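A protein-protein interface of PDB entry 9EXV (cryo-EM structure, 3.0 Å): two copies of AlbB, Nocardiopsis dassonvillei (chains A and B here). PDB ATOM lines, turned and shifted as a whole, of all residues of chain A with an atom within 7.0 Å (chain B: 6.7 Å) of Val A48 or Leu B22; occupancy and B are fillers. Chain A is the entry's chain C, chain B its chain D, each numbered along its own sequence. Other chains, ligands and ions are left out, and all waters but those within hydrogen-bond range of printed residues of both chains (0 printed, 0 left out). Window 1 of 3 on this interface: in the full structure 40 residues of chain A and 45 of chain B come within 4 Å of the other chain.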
ATOM      1  N   LEU A  15       4.907 -28.476 -21.943  1.00  0.00           N
ATOM      2  CA  LEU A  15       4.682 -27.244 -21.196  1.00  0.00           C
ATOM      3  C   LEU A  15       5.944 -26.395 -21.133  1.00  0.00           C
ATOM      4  O   LEU A  15       5.879 -25.165 -21.242  1.00  0.00           O
ATOM      5  CB  LEU A  15       4.188 -27.561 -19.788  1.00  0.00           C
ATOM      6  CG  LEU A  15       2.710 -27.922 -19.662  1.00  0.00           C
ATOM      7  CD1 LEU A  15       2.405 -28.434 -18.266  1.00  0.00           C
ATOM      8  CD2 LEU A  15       1.848 -26.716 -19.992  1.00  0.00           C
ATOM      9  N   LEU A  18       6.296 -24.687 -24.375  1.00  0.00           N
ATOM     10  CA  LEU A  18       5.339 -23.592 -24.486  1.00  0.00           C
ATOM     11  C   LEU A  18       5.794 -22.377 -23.687  1.00  0.00           C
ATOM     12  O   LEU A  18       5.624 -21.235 -24.132  1.00  0.00           O
ATOM     13  CB  LEU A  18       3.957 -24.057 -24.025  1.00  0.00           C
ATOM     14  CG  LEU A  18       2.796 -23.095 -24.282  1.00  0.00           C
ATOM     15  CD1 LEU A  18       1.516 -23.876 -24.473  1.00  0.00           C
ATOM     16  CD2 LEU A  18       2.633 -22.093 -23.149  1.00  0.00           C
ATOM     17  N   LEU A  22       6.511 -18.625 -24.976  1.00  0.00           N
ATOM     18  CA  LEU A  22       5.941 -17.416 -24.393  1.00  0.00           C
ATOM     19  C   LEU A  22       7.020 -16.386 -24.095  1.00  0.00           C
ATOM     20  O   LEU A  22       6.839 -15.192 -24.357  1.00  0.00           O
ATOM     21  CB  LEU A  22       5.161 -17.762 -23.124  1.00  0.00           C
ATOM     22  CG  LEU A  22       3.695 -18.135 -23.342  1.00  0.00           C
ATOM     23  CD1 LEU A  22       3.126 -18.816 -22.112  1.00  0.00           C
ATOM     24  CD2 LEU A  22       2.880 -16.900 -23.692  1.00  0.00           C
ATOM     25  N   THR A  38      -1.834  -9.061 -29.191  1.00  0.00           N
ATOM     26  CA  THR A  38      -3.040  -9.876 -29.130  1.00  0.00           C
ATOM     27  C   THR A  38      -2.892 -11.142 -29.960  1.00  0.00           C
ATOM     28  O   THR A  38      -3.373 -12.211 -29.567  1.00  0.00           O
ATOM     29  CB  THR A  38      -4.245  -9.071 -29.606  1.00  0.00           C
ATOM     30  OG1 THR A  38      -4.444  -7.967 -28.723  1.00  0.00           O
ATOM     31  CG2 THR A  38      -5.490  -9.940 -29.628  1.00  0.00           C
ATOM     32  N   ARG A  40      -0.092 -12.771 -30.644  1.00  0.00           N
ATOM     33  CA  ARG A  40       0.782 -13.703 -29.942  1.00  0.00           C
ATOM     34  C   ARG A  40       0.054 -14.356 -28.775  1.00  0.00           C
ATOM     35  O   ARG A  40       0.220 -15.554 -28.523  1.00  0.00           O
ATOM     36  CB  ARG A  40       2.046 -12.977 -29.492  1.00  0.00           C
ATOM     37  CG  ARG A  40       2.888 -12.452 -30.652  1.00  0.00           C
ATOM     38  CD  ARG A  40       3.655 -13.562 -31.351  1.00  0.00           C
ATOM     39  NE  ARG A  40       5.026 -13.158 -31.643  1.00  0.00           N
ATOM     40  CZ  ARG A  40       5.397 -12.462 -32.710  1.00  0.00           C
ATOM     41  NH1 ARG A  40       4.520 -12.079 -33.623  1.00  0.00           N
ATOM     42  NH2 ARG A  40       6.677 -12.139 -32.859  1.00  0.00           N
ATOM     43  N   CYS A  41      -0.787 -13.593 -28.073  1.00  0.00           N
ATOM     44  CA  CYS A  41      -1.614 -14.178 -27.024  1.00  0.00           C
ATOM     45  C   CYS A  41      -2.563 -15.231 -27.588  1.00  0.00           C
ATOM     46  O   CYS A  41      -2.723 -16.310 -27.004  1.00  0.00           O
ATOM     47  CB  CYS A  41      -2.394 -13.083 -26.298  1.00  0.00           C
ATOM     48  N   LEU A  42      -3.200 -14.935 -28.724  1.00  0.00           N
ATOM     49  CA  LEU A  42      -4.135 -15.875 -29.341  1.00  0.00           C
ATOM     50  C   LEU A  42      -3.417 -17.123 -29.845  1.00  0.00           C
ATOM     51  O   LEU A  42      -3.933 -18.241 -29.725  1.00  0.00           O
ATOM     52  CB  LEU A  42      -4.880 -15.165 -30.473  1.00  0.00           C
ATOM     53  CG  LEU A  42      -6.114 -15.800 -31.112  1.00  0.00           C
ATOM     54  CD1 LEU A  42      -7.094 -14.723 -31.531  1.00  0.00           C
ATOM     55  CD2 LEU A  42      -5.741 -16.618 -32.305  1.00  0.00           C
ATOM     56  N   ASP A  43      -2.230 -16.940 -30.421  1.00  0.00           N
ATOM     57  CA  ASP A  43      -1.401 -18.068 -30.833  1.00  0.00           C
ATOM     58  C   ASP A  43      -1.081 -18.964 -29.645  1.00  0.00           C
ATOM     59  O   ASP A  43      -1.218 -20.189 -29.716  1.00  0.00           O
ATOM     60  CB  ASP A  43      -0.115 -17.544 -31.472  1.00  0.00           C
ATOM     61  CG  ASP A  43       0.708 -18.633 -32.120  1.00  0.00           C
ATOM     62  OD1 ASP A  43       0.169 -19.736 -32.342  1.00  0.00           O
ATOM     63  OD2 ASP A  43       1.898 -18.386 -32.407  1.00  0.00           O
ATOM     64  N   ALA A  44      -0.659 -18.363 -28.535  1.00  0.00           N
ATOM     65  CA  ALA A  44      -0.396 -19.137 -27.328  1.00  0.00           C
ATOM     66  C   ALA A  44      -1.658 -19.835 -26.842  1.00  0.00           C
ATOM     67  O   ALA A  44      -1.596 -20.960 -26.334  1.00  0.00           O
ATOM     68  CB  ALA A  44       0.174 -18.231 -26.239  1.00  0.00           C
ATOM     69  N   ALA A  45      -2.810 -19.177 -26.981  1.00  0.00           N
ATOM     70  CA  ALA A  45      -4.070 -19.789 -26.576  1.00  0.00           C
ATOM     71  C   ALA A  45      -4.325 -21.076 -27.347  1.00  0.00           C
ATOM     72  O   ALA A  45      -4.642 -22.116 -26.758  1.00  0.00           O
ATOM     73  CB  ALA A  45      -5.221 -18.805 -26.784  1.00  0.00           C
ATOM     74  N   ARG A  46      -4.184 -21.031 -28.674  1.00  0.00           N
ATOM     75  CA  ARG A  46      -4.425 -22.235 -29.455  1.00  0.00           C
ATOM     76  C   ARG A  46      -3.364 -23.295 -29.195  1.00  0.00           C
ATOM     77  O   ARG A  46      -3.672 -24.490 -29.231  1.00  0.00           O
ATOM     78  CB  ARG A  46      -4.514 -21.911 -30.949  1.00  0.00           C
ATOM     79  CG  ARG A  46      -3.356 -21.134 -31.529  1.00  0.00           C
ATOM     80  CD  ARG A  46      -3.409 -21.146 -33.045  1.00  0.00           C
ATOM     81  NE  ARG A  46      -3.032 -22.449 -33.583  1.00  0.00           N
ATOM     82  CZ  ARG A  46      -1.813 -22.765 -33.998  1.00  0.00           C
ATOM     83  NH1 ARG A  46      -0.825 -21.886 -33.979  1.00  0.00           N
ATOM     84  NH2 ARG A  46      -1.579 -23.996 -34.443  1.00  0.00           N
ATOM     85  N   ARG A  47      -2.120 -22.894 -28.921  1.00  0.00           N
ATOM     86  CA  ARG A  47      -1.102 -23.873 -28.554  1.00  0.00           C
ATOM     87  C   ARG A  47      -1.463 -24.585 -27.252  1.00  0.00           C
ATOM     88  O   ARG A  47      -1.343 -25.811 -27.150  1.00  0.00           O
ATOM     89  CB  ARG A  47       0.261 -23.188 -28.444  1.00  0.00           C
ATOM     90  CG  ARG A  47       0.780 -22.649 -29.773  1.00  0.00           C
ATOM     91  CD  ARG A  47       2.075 -21.864 -29.617  1.00  0.00           C
ATOM     92  NE  ARG A  47       2.532 -21.323 -30.893  1.00  0.00           N
ATOM     93  CZ  ARG A  47       3.236 -22.002 -31.789  1.00  0.00           C
ATOM     94  NH1 ARG A  47       3.594 -23.258 -31.579  1.00  0.00           N
ATOM     95  NH2 ARG A  47       3.587 -21.407 -32.925  1.00  0.00           N
ATOM     96  N   VAL A  48      -1.918 -23.829 -26.250  1.00  0.00           N
ATOM     97  CA  VAL A  48      -2.334 -24.427 -24.986  1.00  0.00           C
ATOM     98  C   VAL A  48      -3.498 -25.382 -25.206  1.00  0.00           C
ATOM     99  O   VAL A  48      -3.533 -26.485 -24.647  1.00  0.00           O
ATOM    100  CB  VAL A  48      -2.694 -23.330 -23.968  1.00  0.00           C
ATOM    101  CG1 VAL A  48      -3.383 -23.933 -22.756  1.00  0.00           C
ATOM    102  CG2 VAL A  48      -1.459 -22.559 -23.545  1.00  0.00           C
ATOM    103  N   LEU A  49      -4.477 -24.970 -26.011  1.00  0.00           N
ATOM    104  CA  LEU A  49      -5.598 -25.850 -26.308  1.00  0.00           C
ATOM    105  C   LEU A  49      -5.147 -27.096 -27.056  1.00  0.00           C
ATOM    106  O   LEU A  49      -5.744 -28.166 -26.893  1.00  0.00           O
ATOM    107  CB  LEU A  49      -6.661 -25.100 -27.106  1.00  0.00           C
ATOM    108  CG  LEU A  49      -7.387 -24.004 -26.327  1.00  0.00           C
ATOM    109  CD1 LEU A  49      -8.304 -23.219 -27.243  1.00  0.00           C
ATOM    110  CD2 LEU A  49      -8.170 -24.598 -25.164  1.00  0.00           C
ATOM    111  N   ALA A  50      -4.105 -26.979 -27.881  1.00  0.00           N
ATOM    112  CA  ALA A  50      -3.541 -28.164 -28.518  1.00  0.00           C
ATOM    113  C   ALA A  50      -2.990 -29.128 -27.477  1.00  0.00           C
ATOM    114  O   ALA A  50      -3.212 -30.341 -27.564  1.00  0.00           O
ATOM    115  CB  ALA A  50      -2.447 -27.766 -29.506  1.00  0.00           C
ATOM    116  N   LEU A  51      -2.271 -28.607 -26.481  1.00  0.00           N
ATOM    117  CA  LEU A  51      -1.765 -29.469 -25.423  1.00  0.00           C
ATOM    118  C   LEU A  51      -2.905 -30.131 -24.664  1.00  0.00           C
ATOM    119  O   LEU A  51      -2.826 -31.317 -24.321  1.00  0.00           O
ATOM    120  CB  LEU A  51      -0.878 -28.675 -24.465  1.00  0.00           C
ATOM    121  CG  LEU A  51       0.235 -27.857 -25.116  1.00  0.00           C
ATOM    122  CD1 LEU A  51       1.177 -27.307 -24.063  1.00  0.00           C
ATOM    123  CD2 LEU A  51       0.991 -28.689 -26.141  1.00  0.00           C
ATOM    124  N   ALA A  52      -3.977 -29.388 -24.396  1.00  0.00           N
ATOM    125  CA  ALA A  52      -5.104 -29.912 -23.638  1.00  0.00           C
ATOM    126  C   ALA A  52      -6.077 -30.721 -24.486  1.00  0.00           C
ATOM    127  O   ALA A  52      -7.048 -31.255 -23.940  1.00  0.00           O
ATOM    128  CB  ALA A  52      -5.857 -28.769 -22.952  1.00  0.00           C
ATOM    129  N   ALA A  53      -5.854 -30.816 -25.798  1.00  0.00           N
ATOM    130  CA  ALA A  53      -6.787 -31.538 -26.656  1.00  0.00           C
ATOM    131  C   ALA A  53      -6.753 -33.038 -26.387  1.00  0.00           C
ATOM    132  O   ALA A  53      -7.799 -33.697 -26.387  1.00  0.00           O
ATOM    133  CB  ALA A  53      -6.480 -31.250 -28.124  1.00  0.00           C
ATOM    134  N   LEU A  86     -11.627 -11.709 -30.676  1.00  0.00           N
ATOM    135  CA  LEU A  86     -11.161 -12.122 -29.356  1.00  0.00           C
ATOM    136  C   LEU A  86     -12.309 -12.184 -28.360  1.00  0.00           C
ATOM    137  O   LEU A  86     -12.401 -13.128 -27.572  1.00  0.00           O
ATOM    138  CB  LEU A  86     -10.071 -11.174 -28.862  1.00  0.00           C
ATOM    139  CG  LEU A  86      -8.638 -11.467 -29.305  1.00  0.00           C
ATOM    140  CD1 LEU A  86      -8.162 -12.782 -28.710  1.00  0.00           C
ATOM    141  CD2 LEU A  86      -8.514 -11.490 -30.809  1.00  0.00           C
ATOM    142  N   GLU B  14      -6.454 -27.278 -15.576  1.00  0.00           N
ATOM    143  CA  GLU B  14      -5.661 -26.074 -15.400  1.00  0.00           C
ATOM    144  C   GLU B  14      -5.203 -25.514 -16.738  1.00  0.00           C
ATOM    145  O   GLU B  14      -5.052 -24.296 -16.880  1.00  0.00           O
ATOM    146  CB  GLU B  14      -4.478 -26.357 -14.473  1.00  0.00           C
ATOM    147  CG  GLU B  14      -4.912 -26.638 -13.040  1.00  0.00           C
ATOM    148  CD  GLU B  14      -3.753 -26.893 -12.101  1.00  0.00           C
ATOM    149  OE1 GLU B  14      -2.616 -27.003 -12.580  1.00  0.00           O
ATOM    150  OE2 GLU B  14      -3.983 -26.981 -10.878  1.00  0.00           O
ATOM    151  N   LEU B  15      -5.003 -26.379 -17.736  1.00  0.00           N
ATOM    152  CA  LEU B  15      -4.695 -25.898 -19.080  1.00  0.00           C
ATOM    153  C   LEU B  15      -5.860 -25.117 -19.669  1.00  0.00           C
ATOM    154  O   LEU B  15      -5.656 -24.102 -20.348  1.00  0.00           O
ATOM    155  CB  LEU B  15      -4.334 -27.067 -19.991  1.00  0.00           C
ATOM    156  CG  LEU B  15      -2.979 -27.726 -19.744  1.00  0.00           C
ATOM    157  CD1 LEU B  15      -2.812 -28.949 -20.629  1.00  0.00           C
ATOM    158  CD2 LEU B  15      -1.856 -26.731 -19.977  1.00  0.00           C
ATOM    159  N   LEU B  16      -7.090 -25.586 -19.450  1.00  0.00           N
ATOM    160  CA  LEU B  16      -8.247 -24.845 -19.930  1.00  0.00           C
ATOM    161  C   LEU B  16      -8.325 -23.471 -19.284  1.00  0.00           C
ATOM    162  O   LEU B  16      -8.566 -22.468 -19.964  1.00  0.00           O
ATOM    163  CB  LEU B  16      -9.528 -25.633 -19.667  1.00  0.00           C
ATOM    164  CG  LEU B  16      -9.949 -26.533 -20.824  1.00  0.00           C
ATOM    165  CD1 LEU B  16      -9.027 -27.728 -20.920  1.00  0.00           C
ATOM    166  CD2 LEU B  16     -11.390 -26.968 -20.682  1.00  0.00           C
ATOM    167  N   LEU B  17      -8.110 -23.397 -17.970  1.00  0.00           N
ATOM    168  CA  LEU B  17      -8.119 -22.103 -17.305  1.00  0.00           C
ATOM    169  C   LEU B  17      -6.991 -21.214 -17.817  1.00  0.00           C
ATOM    170  O   LEU B  17      -7.173 -20.003 -17.985  1.00  0.00           O
ATOM    171  CB  LEU B  17      -8.035 -22.294 -15.791  1.00  0.00           C
ATOM    172  CG  LEU B  17      -9.308 -22.910 -15.208  1.00  0.00           C
ATOM    173  CD1 LEU B  17      -9.038 -23.558 -13.873  1.00  0.00           C
ATOM    174  CD2 LEU B  17     -10.400 -21.856 -15.079  1.00  0.00           C
ATOM    175  N   LEU B  18      -5.822 -21.802 -18.077  1.00  0.00           N
ATOM    176  CA  LEU B  18      -4.707 -21.041 -18.634  1.00  0.00           C
ATOM    177  C   LEU B  18      -5.042 -20.489 -20.014  1.00  0.00           C
ATOM    178  O   LEU B  18      -4.694 -19.347 -20.338  1.00  0.00           O
ATOM    179  CB  LEU B  18      -3.466 -21.929 -18.703  1.00  0.00           C
ATOM    180  CG  LEU B  18      -2.250 -21.373 -19.436  1.00  0.00           C
ATOM    181  CD1 LEU B  18      -1.643 -20.218 -18.660  1.00  0.00           C
ATOM    182  CD2 LEU B  18      -1.233 -22.476 -19.666  1.00  0.00           C
ATOM    183  N   ALA B  19      -5.698 -21.297 -20.850  1.00  0.00           N
ATOM    184  CA  ALA B  19      -6.096 -20.827 -22.173  1.00  0.00           C
ATOM    185  C   ALA B  19      -7.095 -19.686 -22.067  1.00  0.00           C
ATOM    186  O   ALA B  19      -7.033 -18.721 -22.836  1.00  0.00           O
ATOM    187  CB  ALA B  19      -6.681 -21.981 -22.986  1.00  0.00           C
ATOM    188  N   ALA B  20      -8.029 -19.780 -21.120  1.00  0.00           N
ATOM    189  CA  ALA B  20      -8.952 -18.677 -20.894  1.00  0.00           C
ATOM    190  C   ALA B  20      -8.207 -17.418 -20.477  1.00  0.00           C
ATOM    191  O   ALA B  20      -8.533 -16.316 -20.932  1.00  0.00           O
ATOM    192  CB  ALA B  20      -9.989 -19.057 -19.843  1.00  0.00           C
ATOM    193  N   TYR B  21      -7.199 -17.559 -19.612  1.00  0.00           N
ATOM    194  CA  TYR B  21      -6.406 -16.398 -19.222  1.00  0.00           C
ATOM    195  C   TYR B  21      -5.682 -15.795 -20.416  1.00  0.00           C
ATOM    196  O   TYR B  21      -5.617 -14.569 -20.556  1.00  0.00           O
ATOM    197  CB  TYR B  21      -5.400 -16.766 -18.135  1.00  0.00           C
ATOM    198  CG  TYR B  21      -4.242 -15.794 -18.072  1.00  0.00           C
ATOM    199  CD1 TYR B  21      -4.401 -14.529 -17.522  1.00  0.00           C
ATOM    200  CD2 TYR B  21      -2.994 -16.135 -18.578  1.00  0.00           C
ATOM    201  CE1 TYR B  21      -3.349 -13.634 -17.470  1.00  0.00           C
ATOM    202  CE2 TYR B  21      -1.938 -15.247 -18.531  1.00  0.00           C
ATOM    203  CZ  TYR B  21      -2.121 -13.999 -17.976  1.00  0.00           C
ATOM    204  OH  TYR B  21      -1.071 -13.113 -17.928  1.00  0.00           O
ATOM    205  N   LEU B  22      -5.104 -16.641 -21.275  1.00  0.00           N
ATOM    206  CA  LEU B  22      -4.403 -16.128 -22.446  1.00  0.00           C
ATOM    207  C   LEU B  22      -5.352 -15.392 -23.379  1.00  0.00           C
ATOM    208  O   LEU B  22      -5.010 -14.332 -23.916  1.00  0.00           O
ATOM    209  CB  LEU B  22      -3.700 -17.271 -23.178  1.00  0.00           C
ATOM    210  CG  LEU B  22      -2.331 -17.656 -22.616  1.00  0.00           C
ATOM    211  CD1 LEU B  22      -1.888 -19.007 -23.145  1.00  0.00           C
ATOM    212  CD2 LEU B  22      -1.301 -16.588 -22.955  1.00  0.00           C
ATOM    213  N   LEU B  23      -6.552 -15.937 -23.583  1.00  0.00           N
ATOM    214  CA  LEU B  23      -7.542 -15.259 -24.412  1.00  0.00           C
ATOM    215  C   LEU B  23      -7.956 -13.927 -23.807  1.00  0.00           C
ATOM    216  O   LEU B  23      -8.096 -12.926 -24.520  1.00  0.00           O
ATOM    217  CB  LEU B  23      -8.761 -16.152 -24.593  1.00  0.00           C
ATOM    218  CG  LEU B  23      -8.669 -17.119 -25.756  1.00  0.00           C
ATOM    219  CD1 LEU B  23      -9.754 -18.166 -25.607  1.00  0.00           C
ATOM    220  CD2 LEU B  23      -8.804 -16.332 -27.053  1.00  0.00           C
ATOM    221  N   SER B  24      -8.177 -13.902 -22.494  1.00  0.00           N
ATOM    222  CA  SER B  24      -8.540 -12.655 -21.835  1.00  0.00           C
ATOM    223  C   SER B  24      -7.423 -11.631 -21.962  1.00  0.00           C
ATOM    224  O   SER B  24      -7.681 -10.445 -22.190  1.00  0.00           O
ATOM    225  CB  SER B  24      -8.876 -12.918 -20.369  1.00  0.00           C
ATOM    226  OG  SER B  24      -9.275 -11.725 -19.725  1.00  0.00           O
ATOM    227  N   SER B  25      -6.170 -12.073 -21.829  1.00  0.00           N
ATOM    228  CA  SER B  25      -5.044 -11.165 -22.022  1.00  0.00           C
ATOM    229  C   SER B  25      -5.004 -10.634 -23.448  1.00  0.00           C
ATOM    230  O   SER B  25      -4.725  -9.452 -23.671  1.00  0.00           O
ATOM    231  CB  SER B  25      -3.736 -11.874 -21.678  1.00  0.00           C
ATOM    232  OG  SER B  25      -3.696 -12.242 -20.312  1.00  0.00           O
ATOM    233  N   GLY B  26      -5.274 -11.499 -24.427  1.00  0.00           N
ATOM    234  CA  GLY B  26      -5.309 -11.044 -25.805  1.00  0.00           C
ATOM    235  C   GLY B  26      -6.357  -9.973 -26.029  1.00  0.00           C
ATOM    236  O   GLY B  26      -6.089  -8.946 -26.656  1.00  0.00           O
ATOM    237  N   ARG B  27      -7.566 -10.191 -25.508  1.00  0.00           N
ATOM    238  CA  ARG B  27      -8.596  -9.167 -25.630  1.00  0.00           C
ATOM    239  C   ARG B  27      -8.201  -7.902 -24.883  1.00  0.00           C
ATOM    240  O   ARG B  27      -8.431  -6.787 -25.369  1.00  0.00           O
ATOM    241  CB  ARG B  27      -9.938  -9.692 -25.117  1.00  0.00           C
ATOM    242  CG  ARG B  27     -11.058  -8.649 -25.147  1.00  0.00           C
ATOM    243  CD  ARG B  27     -11.161  -7.969 -26.511  1.00  0.00           C
ATOM    244  NE  ARG B  27     -12.270  -7.024 -26.582  1.00  0.00           N
ATOM    245  CZ  ARG B  27     -12.218  -5.769 -26.159  1.00  0.00           C
ATOM    246  NH1 ARG B  27     -11.119  -5.264 -25.628  1.00  0.00           N
ATOM    247  NH2 ARG B  27     -13.301  -5.003 -26.268  1.00  0.00           N
ATOM    248  N   ARG B  40       2.355  -9.477 -20.134  1.00  0.00           N
ATOM    249  CA  ARG B  40       1.376 -10.559 -20.106  1.00  0.00           C
ATOM    250  C   ARG B  40       2.001 -11.875 -20.550  1.00  0.00           C
ATOM    251  O   ARG B  40       1.677 -12.937 -20.007  1.00  0.00           O
ATOM    252  CB  ARG B  40       0.173 -10.199 -20.972  1.00  0.00           C
ATOM    253  CG  ARG B  40      -0.621  -9.021 -20.432  1.00  0.00           C
ATOM    254  CD  ARG B  40      -1.348  -9.379 -19.143  1.00  0.00           C
ATOM    255  NE  ARG B  40      -1.799  -8.191 -18.428  1.00  0.00           N
ATOM    256  CZ  ARG B  40      -2.869  -7.480 -18.754  1.00  0.00           C
ATOM    257  NH1 ARG B  40      -3.626  -7.806 -19.791  1.00  0.00           N
ATOM    258  NH2 ARG B  40      -3.187  -6.414 -18.027  1.00  0.00           N
ATOM    259  N   CYS B  41       2.902 -11.824 -21.532  1.00  0.00           N
ATOM    260  CA  CYS B  41       3.619 -13.029 -21.931  1.00  0.00           C
ATOM    261  C   CYS B  41       4.457 -13.573 -20.780  1.00  0.00           C
ATOM    262  O   CYS B  41       4.507 -14.789 -20.559  1.00  0.00           O
ATOM    263  CB  CYS B  41       4.495 -12.743 -23.149  1.00  0.00           C
ATOM    264  N   ALA B  44       2.089 -15.202 -18.231  1.00  0.00           N
ATOM    265  CA  ALA B  44       1.680 -16.512 -18.722  1.00  0.00           C
ATOM    266  C   ALA B  44       2.827 -17.506 -18.649  1.00  0.00           C
ATOM    267  O   ALA B  44       2.615 -18.689 -18.364  1.00  0.00           O
ATOM    268  CB  ALA B  44       1.159 -16.394 -20.153  1.00  0.00           C
ATOM    269  N   ARG B  47       3.115 -18.689 -15.100  1.00  0.00           N
ATOM    270  CA  ARG B  47       2.001 -19.591 -14.824  1.00  0.00           C
ATOM    271  C   ARG B  47       2.256 -20.968 -15.421  1.00  0.00           C
ATOM    272  O   ARG B  47       2.065 -21.994 -14.760  1.00  0.00           O
ATOM    273  CB  ARG B  47       0.703 -18.998 -15.373  1.00  0.00           C
ATOM    274  CG  ARG B  47       0.212 -17.775 -14.619  1.00  0.00           C
ATOM    275  CD  ARG B  47      -0.589 -16.849 -15.521  1.00  0.00           C
ATOM    276  NE  ARG B  47      -1.296 -15.825 -14.760  1.00  0.00           N
ATOM    277  CZ  ARG B  47      -2.613 -15.773 -14.597  1.00  0.00           C
ATOM    278  NH1 ARG B  47      -3.416 -16.663 -15.155  1.00  0.00           N
ATOM    279  NH2 ARG B  47      -3.135 -14.797 -13.859  1.00  0.00           N
ATOM    280  N   VAL B  48       2.702 -21.005 -16.680  1.00  0.00           N
ATOM    281  CA  VAL B  48       2.986 -22.276 -17.337  1.00  0.00           C
ATOM    282  C   VAL B  48       4.107 -23.006 -16.618  1.00  0.00           C
ATOM    283  O   VAL B  48       4.085 -24.236 -16.488  1.00  0.00           O
ATOM    284  CB  VAL B  48       3.329 -22.062 -18.822  1.00  0.00           C
ATOM    285  CG1 VAL B  48       3.785 -23.373 -19.447  1.00  0.00           C
ATOM    286  CG2 VAL B  48       2.141 -21.508 -19.573  1.00  0.00           C
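The side-chain hydroxyl (OG1) of Thr A38 is in hydrogen-bond range of the backbone carbonyl oxygen (O) of Gly B26 (2.8 Å).
Among the printed residues, pairs that only touch across the chains: Leu A15 with Val B48 (3.3 Å), Val A48 with Leu B15 (3.3 Å), Cys A41 with Gly B26 (3.6 Å), Leu A22 with Cys B41 (3.6 Å), Val A48 with Leu B22 (3.6 Å), Leu A18 with Val B48 (3.7 Å), Leu A22 with Ala B44 (3.7 Å), Leu A15 with Leu B15 (3.7 Å), Leu A49 with Ala B19 (3.7 Å), Ala A52 with Leu B15 (3.7 Å), Ala A44 with Leu B22 (3.8 Å), Cys A41 with Leu B22 (3.8 Å), Leu A22 with Val B48 (3.8 Å), Val A48 with Ala B19 (3.8 Å), Val A48 with Leu B18 (3.9 Å), Ala A52 with Leu B16 (3.9 Å), Ala A45 with Leu B22 (3.9 Å), Leu A86 with Leu B23 (3.97 Å) and Ala A45 with Leu B23 (3.97 Å).
Of chain B, only Leu B15 (3.3 Å), Leu B18 (3.9 Å), Ala B19 (3.8 Å) and Leu B22 (3.6 Å) come within 4 Å of Val A48. Leu B22 touches just these residues of chain A: Cys A41, Ala A44, Ala A45 and Val A48. Of the printed residues of chain B, Thr A38 touches Gly B26 (2.8 Å). Of the printed residues of chain A, Gly B26 touches Thr A38 (2.8 Å) and Cys A41 (3.6 Å). Arg B40 touches none of the printed residues of chain A. The nearest residue of chain A that does not touch Leu B22 is Leu A22 (4.3 Å).
Hydrophobic or aromatic side chains of chain B that line the printed part of chain A: Leu B15, Leu B16, Leu B18, Ala B19, Leu B22, Leu B23, Ala B44 and Val B48. Of the 19 printed residues of chain A, 11 touch a printed residue of chain B. Hydrophobic or aromatic side chains of chain A that line the printed part of chain B: Leu A15, Leu A18, Leu A22, Ala A44, Ala A45, Val A48, Leu A49, Ala A52 and Leu A86.
Leu A15 touches Val B48, and with the chains exchanged Val A48 touches Leu B15. Leu A18 touches Val B48, and with the chains exchanged Val A48 touches Leu B18. Leu A22 touches Cys B41, and with the chains exchanged Cys A41 touches Leu B22. Leu A22 touches Val B48, and with the chains exchanged Val A48 touches Leu B22.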
